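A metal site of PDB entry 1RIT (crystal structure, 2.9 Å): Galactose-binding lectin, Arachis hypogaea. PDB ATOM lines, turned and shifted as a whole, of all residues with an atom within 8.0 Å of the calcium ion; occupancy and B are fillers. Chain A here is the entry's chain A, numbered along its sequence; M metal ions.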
ATOM      1  N   PRO A  81     -11.086  -4.806 -11.460  1.00  0.00           N
ATOM      2  CA  PRO A  81     -11.194  -4.541 -10.017  1.00  0.00           C
ATOM      3  C   PRO A  81     -10.967  -5.799  -9.199  1.00  0.00           C
ATOM      4  O   PRO A  81     -11.790  -6.704  -9.191  1.00  0.00           O
ATOM      5  CB  PRO A  81     -12.619  -4.018  -9.883  1.00  0.00           C
ATOM      6  CG  PRO A  81     -12.801  -3.261 -11.152  1.00  0.00           C
ATOM      7  CD  PRO A  81     -12.228  -4.218 -12.183  1.00  0.00           C
ATOM      8  N   ALA A  82      -9.836  -5.827  -8.505  1.00  0.00           N
ATOM      9  CA  ALA A  82      -9.457  -6.966  -7.666  1.00  0.00           C
ATOM     10  C   ALA A  82      -8.325  -6.583  -6.707  1.00  0.00           C
ATOM     11  O   ALA A  82      -7.711  -5.520  -6.864  1.00  0.00           O
ATOM     12  CB  ALA A  82      -9.039  -8.133  -8.551  1.00  0.00           C
ATOM     13  N   ASP A  83      -8.040  -7.427  -5.712  1.00  0.00           N
ATOM     14  CA  ASP A  83      -8.763  -8.675  -5.441  1.00  0.00           C
ATOM     15  C   ASP A  83      -9.879  -8.504  -4.425  1.00  0.00           C
ATOM     16  O   ASP A  83     -10.808  -9.295  -4.390  1.00  0.00           O
ATOM     17  CB  ASP A  83      -7.810  -9.723  -4.920  1.00  0.00           C
ATOM     18  CG  ASP A  83      -7.210 -10.539  -6.003  1.00  0.00           C
ATOM     19  OD1 ASP A  83      -7.990 -11.249  -6.666  1.00  0.00           O
ATOM     20  OD2 ASP A  83      -5.987 -10.472  -6.183  1.00  0.00           O
ATOM     21  N   GLY A  84      -9.767  -7.456  -3.606  1.00  0.00           N
ATOM     22  CA  GLY A  84     -10.767  -7.195  -2.580  1.00  0.00           C
ATOM     23  C   GLY A  84     -10.074  -7.066  -1.242  1.00  0.00           C
ATOM     24  O   GLY A  84      -8.877  -7.319  -1.140  1.00  0.00           O
ATOM     25  N   GLY A 102      -1.437 -13.749 -11.107  1.00  0.00           N
ATOM     26  CA  GLY A 102      -2.753 -13.661 -11.684  1.00  0.00           C
ATOM     27  C   GLY A 102      -3.655 -13.792 -10.471  1.00  0.00           C
ATOM     28  O   GLY A 102      -4.700 -13.158 -10.343  1.00  0.00           O
ATOM     29  N   GLY A 103      -3.166 -14.627  -9.560  1.00  0.00           N
ATOM     30  CA  GLY A 103      -3.805 -14.981  -8.306  1.00  0.00           C
ATOM     31  C   GLY A 103      -4.620 -13.974  -7.518  1.00  0.00           C
ATOM     32  O   GLY A 103      -4.593 -12.773  -7.776  1.00  0.00           O
ATOM     33  N   GLY A 104      -5.348 -14.509  -6.541  1.00  0.00           N
ATOM     34  CA  GLY A 104      -6.196 -13.696  -5.693  1.00  0.00           C
ATOM     35  C   GLY A 104      -6.325 -14.376  -4.344  1.00  0.00           C
ATOM     36  O   GLY A 104      -7.403 -14.820  -3.934  1.00  0.00           O
ATOM     37  N   THR A 105      -5.192 -14.440  -3.652  1.00  0.00           N
ATOM     38  CA  THR A 105      -5.101 -15.046  -2.341  1.00  0.00           C
ATOM     39  C   THR A 105      -5.473 -14.047  -1.264  1.00  0.00           C
ATOM     40  O   THR A 105      -5.424 -14.357  -0.078  1.00  0.00           O
ATOM     41  CB  THR A 105      -3.669 -15.537  -2.065  1.00  0.00           C
ATOM     42  OG1 THR A 105      -2.751 -14.458  -2.309  1.00  0.00           O
ATOM     43  CG2 THR A 105      -3.317 -16.715  -2.951  1.00  0.00           C
ATOM     44  N   LEU A 106      -5.851 -12.843  -1.677  1.00  0.00           N
ATOM     45  CA  LEU A 106      -6.207 -11.788  -0.733  1.00  0.00           C
ATOM     46  C   LEU A 106      -5.126 -11.549   0.324  1.00  0.00           C
ATOM     47  O   LEU A 106      -5.404 -10.998   1.388  1.00  0.00           O
ATOM     48  CB  LEU A 106      -7.548 -12.116  -0.063  1.00  0.00           C
ATOM     49  CG  LEU A 106      -8.794 -12.041  -0.959  1.00  0.00           C
ATOM     50  CD1 LEU A 106     -10.065 -12.321  -0.146  1.00  0.00           C
ATOM     51  CD2 LEU A 106      -8.856 -10.663  -1.606  1.00  0.00           C
ATOM     52  N   GLU A 121     -14.266 -12.028   4.010  1.00  0.00           N
ATOM     53  CA  GLU A 121     -13.743 -11.419   2.793  1.00  0.00           C
ATOM     54  C   GLU A 121     -14.782 -10.630   2.028  1.00  0.00           C
ATOM     55  O   GLU A 121     -15.969 -10.965   2.016  1.00  0.00           O
ATOM     56  CB  GLU A 121     -13.162 -12.474   1.877  1.00  0.00           C
ATOM     57  CG  GLU A 121     -14.210 -13.384   1.318  1.00  0.00           C
ATOM     58  CD  GLU A 121     -13.667 -14.292   0.245  1.00  0.00           C
ATOM     59  OE1 GLU A 121     -12.725 -15.057   0.547  1.00  0.00           O
ATOM     60  OE2 GLU A 121     -14.168 -14.247  -0.891  1.00  0.00           O
ATOM     61  N   PHE A 122     -14.307  -9.584   1.367  1.00  0.00           N
ATOM     62  CA  PHE A 122     -15.139  -8.696   0.558  1.00  0.00           C
ATOM     63  C   PHE A 122     -14.514  -8.749  -0.826  1.00  0.00           C
ATOM     64  O   PHE A 122     -13.915  -7.788  -1.308  1.00  0.00           O
ATOM     65  CB  PHE A 122     -15.111  -7.282   1.149  1.00  0.00           C
ATOM     66  CG  PHE A 122     -15.781  -7.195   2.497  1.00  0.00           C
ATOM     67  CD1 PHE A 122     -17.045  -6.629   2.626  1.00  0.00           C
ATOM     68  CD2 PHE A 122     -15.176  -7.721   3.629  1.00  0.00           C
ATOM     69  CE1 PHE A 122     -17.691  -6.613   3.856  1.00  0.00           C
ATOM     70  CE2 PHE A 122     -15.822  -7.705   4.858  1.00  0.00           C
ATOM     71  CZ  PHE A 122     -17.075  -7.152   4.973  1.00  0.00           C
ATOM     72  N   ASP A 123     -14.665  -9.915  -1.444  1.00  0.00           N
ATOM     73  CA  ASP A 123     -14.148 -10.255  -2.772  1.00  0.00           C
ATOM     74  C   ASP A 123     -14.887  -9.649  -3.965  1.00  0.00           C
ATOM     75  O   ASP A 123     -16.108  -9.791  -4.067  1.00  0.00           O
ATOM     76  CB  ASP A 123     -14.175 -11.774  -2.900  1.00  0.00           C
ATOM     77  CG  ASP A 123     -13.440 -12.269  -4.113  1.00  0.00           C
ATOM     78  OD1 ASP A 123     -13.051 -11.456  -4.988  1.00  0.00           O
ATOM     79  OD2 ASP A 123     -13.258 -13.500  -4.194  1.00  0.00           O
ATOM     80  N   THR A 124     -14.151  -9.032  -4.894  1.00  0.00           N
ATOM     81  CA  THR A 124     -14.740  -8.404  -6.070  1.00  0.00           C
ATOM     82  C   THR A 124     -14.338  -8.996  -7.443  1.00  0.00           C
ATOM     83  O   THR A 124     -14.584  -8.369  -8.507  1.00  0.00           O
ATOM     84  CB  THR A 124     -14.428  -6.882  -6.095  1.00  0.00           C
ATOM     85  OG1 THR A 124     -13.031  -6.683  -6.328  1.00  0.00           O
ATOM     86  CG2 THR A 124     -14.803  -6.228  -4.766  1.00  0.00           C
ATOM     87  N   TYR A 125     -13.765 -10.190  -7.439  1.00  0.00           N
ATOM     88  CA  TYR A 125     -13.341 -10.824  -8.692  1.00  0.00           C
ATOM     89  C   TYR A 125     -13.331 -12.352  -8.602  1.00  0.00           C
ATOM     90  O   TYR A 125     -12.650 -12.912  -7.754  1.00  0.00           O
ATOM     91  CB  TYR A 125     -11.972 -10.300  -9.078  1.00  0.00           C
ATOM     92  CG  TYR A 125     -11.351 -10.979 -10.271  1.00  0.00           C
ATOM     93  CD1 TYR A 125     -10.655 -12.171 -10.126  1.00  0.00           C
ATOM     94  CD2 TYR A 125     -11.431 -10.399 -11.531  1.00  0.00           C
ATOM     95  CE1 TYR A 125     -10.031 -12.776 -11.222  1.00  0.00           C
ATOM     96  CE2 TYR A 125     -10.816 -11.002 -12.629  1.00  0.00           C
ATOM     97  CZ  TYR A 125     -10.122 -12.185 -12.467  1.00  0.00           C
ATOM     98  OH  TYR A 125      -9.507 -12.737 -13.560  1.00  0.00           O
ATOM     99  N   SER A 126     -14.073 -13.012  -9.485  1.00  0.00           N
ATOM    100  CA  SER A 126     -14.171 -14.476  -9.490  1.00  0.00           C
ATOM    101  C   SER A 126     -12.968 -15.235 -10.061  1.00  0.00           C
ATOM    102  O   SER A 126     -12.426 -14.874 -11.100  1.00  0.00           O
ATOM    103  CB  SER A 126     -15.452 -14.895 -10.239  1.00  0.00           C
ATOM    104  OG  SER A 126     -15.634 -16.306 -10.157  1.00  0.00           O
ATOM    105  N   ASN A 127     -12.574 -16.300  -9.366  1.00  0.00           N
ATOM    106  CA  ASN A 127     -11.446 -17.117  -9.785  1.00  0.00           C
ATOM    107  C   ASN A 127     -11.869 -18.569  -9.756  1.00  0.00           C
ATOM    108  O   ASN A 127     -11.979 -19.157  -8.675  1.00  0.00           O
ATOM    109  CB  ASN A 127     -10.245 -16.982  -8.840  1.00  0.00           C
ATOM    110  CG  ASN A 127     -10.210 -15.662  -8.080  1.00  0.00           C
ATOM    111  OD1 ASN A 127     -11.172 -15.332  -7.377  1.00  0.00           O
ATOM    112  ND2 ASN A 127      -9.106 -14.928  -8.188  1.00  0.00           N
ATOM    113  N   SER A 128     -12.125 -19.144 -10.917  1.00  0.00           N
ATOM    114  CA  SER A 128     -12.523 -20.538 -11.009  1.00  0.00           C
ATOM    115  C   SER A 128     -11.636 -21.390 -10.087  1.00  0.00           C
ATOM    116  O   SER A 128     -12.085 -22.392  -9.529  1.00  0.00           O
ATOM    117  CB  SER A 128     -12.373 -21.021 -12.450  1.00  0.00           C
ATOM    118  OG  SER A 128     -11.052 -20.822 -12.923  1.00  0.00           O
ATOM    119  N   GLU A 129     -10.396 -20.939  -9.927  1.00  0.00           N
ATOM    120  CA  GLU A 129      -9.384 -21.623  -9.119  1.00  0.00           C
ATOM    121  C   GLU A 129      -9.688 -21.793  -7.628  1.00  0.00           C
ATOM    122  O   GLU A 129      -9.130 -22.673  -6.983  1.00  0.00           O
ATOM    123  CB  GLU A 129      -8.037 -20.923  -9.294  1.00  0.00           C
ATOM    124  CG  GLU A 129      -8.075 -19.388  -9.230  1.00  0.00           C
ATOM    125  CD  GLU A 129      -8.257 -18.723 -10.586  1.00  0.00           C
ATOM    126  OE1 GLU A 129      -9.208 -19.081 -11.317  1.00  0.00           O
ATOM    127  OE2 GLU A 129      -7.466 -17.819 -10.920  1.00  0.00           O
ATOM    128  N   TYR A 130     -10.568 -20.959  -7.085  1.00  0.00           N
ATOM    129  CA  TYR A 130     -10.897 -21.049  -5.665  1.00  0.00           C
ATOM    130  C   TYR A 130     -12.399 -21.138  -5.414  1.00  0.00           C
ATOM    131  O   TYR A 130     -12.863 -20.896  -4.302  1.00  0.00           O
ATOM    132  CB  TYR A 130     -10.332 -19.829  -4.912  1.00  0.00           C
ATOM    133  CG  TYR A 130      -8.834 -19.600  -5.057  1.00  0.00           C
ATOM    134  CD1 TYR A 130      -7.915 -20.585  -4.714  1.00  0.00           C
ATOM    135  CD2 TYR A 130      -8.333 -18.384  -5.533  1.00  0.00           C
ATOM    136  CE1 TYR A 130      -6.532 -20.373  -4.841  1.00  0.00           C
ATOM    137  CE2 TYR A 130      -6.965 -18.160  -5.668  1.00  0.00           C
ATOM    138  CZ  TYR A 130      -6.071 -19.157  -5.321  1.00  0.00           C
ATOM    139  OH  TYR A 130      -4.714 -18.948  -5.473  1.00  0.00           O
ATOM    140  N   ASN A 131     -13.162 -21.489  -6.451  1.00  0.00           N
ATOM    141  CA  ASN A 131     -14.626 -21.621  -6.345  1.00  0.00           C
ATOM    142  C   ASN A 131     -15.379 -20.294  -6.226  1.00  0.00           C
ATOM    143  O   ASN A 131     -16.561 -20.279  -5.880  1.00  0.00           O
ATOM    144  CB  ASN A 131     -14.986 -22.515  -5.168  1.00  0.00           C
ATOM    145  CG  ASN A 131     -14.767 -23.990  -5.463  1.00  0.00           C
ATOM    146  OD1 ASN A 131     -13.707 -24.390  -5.953  1.00  0.00           O
ATOM    147  ND2 ASN A 131     -15.764 -24.796  -5.140  1.00  0.00           N
ATOM    148  N   ASP A 132     -14.709 -19.190  -6.514  1.00  0.00           N
ATOM    149  CA  ASP A 132     -15.352 -17.890  -6.436  1.00  0.00           C
ATOM    150  C   ASP A 132     -16.708 -17.848  -7.108  1.00  0.00           C
ATOM    151  O   ASP A 132     -16.820 -18.136  -8.298  1.00  0.00           O
ATOM    152  CB  ASP A 132     -14.479 -16.833  -7.101  1.00  0.00           C
ATOM    153  CG  ASP A 132     -13.523 -16.185  -6.151  1.00  0.00           C
ATOM    154  OD1 ASP A 132     -12.650 -16.895  -5.611  1.00  0.00           O
ATOM    155  OD2 ASP A 132     -13.636 -14.976  -5.946  1.00  0.00           O
ATOM    156  N   PRO A 133     -17.772 -17.516  -6.338  1.00  0.00           N
ATOM    157  CA  PRO A 133     -19.099 -17.462  -6.943  1.00  0.00           C
ATOM    158  C   PRO A 133     -19.037 -16.567  -8.203  1.00  0.00           C
ATOM    159  O   PRO A 133     -18.151 -15.697  -8.322  1.00  0.00           O
ATOM    160  CB  PRO A 133     -19.951 -16.855  -5.830  1.00  0.00           C
ATOM    161  CG  PRO A 133     -19.313 -17.403  -4.601  1.00  0.00           C
ATOM    162  CD  PRO A 133     -17.839 -17.252  -4.890  1.00  0.00           C
ATOM    163  N   HIS A 137     -18.928 -10.985  -3.893  1.00  0.00           N
ATOM    164  CA  HIS A 137     -19.475 -11.657  -2.725  1.00  0.00           C
ATOM    165  C   HIS A 137     -18.768 -11.310  -1.439  1.00  0.00           C
ATOM    166  O   HIS A 137     -17.685 -10.733  -1.450  1.00  0.00           O
ATOM    167  CB  HIS A 137     -19.397 -13.170  -2.924  1.00  0.00           C
ATOM    168  CG  HIS A 137     -18.030 -13.660  -3.292  1.00  0.00           C
ATOM    169  ND1 HIS A 137     -17.471 -13.452  -4.542  1.00  0.00           N
ATOM    170  CD2 HIS A 137     -17.108 -14.341  -2.589  1.00  0.00           C
ATOM    171  CE1 HIS A 137     -16.269 -13.988  -4.569  1.00  0.00           C
ATOM    172  NE2 HIS A 137     -16.020 -14.536  -3.398  1.00  0.00           N
ATOM    173  N   VAL A 145      -9.054 -19.619   1.104  1.00  0.00           N
ATOM    174  CA  VAL A 145      -9.693 -18.516   0.370  1.00  0.00           C
ATOM    175  C   VAL A 145     -10.951 -19.015  -0.377  1.00  0.00           C
ATOM    176  O   VAL A 145     -11.666 -18.210  -0.986  1.00  0.00           O
ATOM    177  CB  VAL A 145      -8.705 -17.853  -0.624  1.00  0.00           C
ATOM    178  CG1 VAL A 145      -7.575 -17.211   0.142  1.00  0.00           C
ATOM    179  CG2 VAL A 145      -8.151 -18.860  -1.629  1.00  0.00           C
ATOM    180  N   SER A 209      -4.800  -7.749  -1.816  1.00  0.00           N
ATOM    181  CA  SER A 209      -3.912  -8.259  -2.853  1.00  0.00           C
ATOM    182  C   SER A 209      -4.358  -7.828  -4.235  1.00  0.00           C
ATOM    183  O   SER A 209      -5.502  -7.418  -4.431  1.00  0.00           O
ATOM    184  CB  SER A 209      -3.898  -9.779  -2.813  1.00  0.00           C
ATOM    185  OG  SER A 209      -5.180 -10.308  -3.131  1.00  0.00           O
HETATM  186 CA    CA M   1     -11.031 -13.640  -5.567  1.00  0.00          CA
HETATM  187 MN    MN M   2     -14.169 -15.819  -2.960  1.00  0.00          MN
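Within 4 Å of the calcium ion: Asp 123, Tyr 125, Asn 127 and Asp 132.
The backbone carbonyl oxygen of Asn 127 is in hydrogen-bond range of the backbone NH of Asp 132. The backbone carbonyl oxygen (O) of Asp 123 sits at hydrogen-bond distance from the backbone NH (N) of His 137 (3.1 Å). The side-chain hydroxyl of Ser 126 sits at hydrogen-bond distance from the backbone carbonyl oxygen of Asp 132.
The calcium ion is bound by the side-chain amide oxygen (OD1) of Asn 127 (2.5 Å), the side-chain carboxylate (OD2) of Asp 123 (2.6 Å) and the backbone carbonyl oxygen (O) of Tyr 125 (2.8 Å). Slightly farther from the calcium ion lies the side-chain carboxylate (OD2) of Asp 132 (3.0 Å). Slightly farther from the calcium ion lies OD1 of Asp 123 (3.0 Å).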
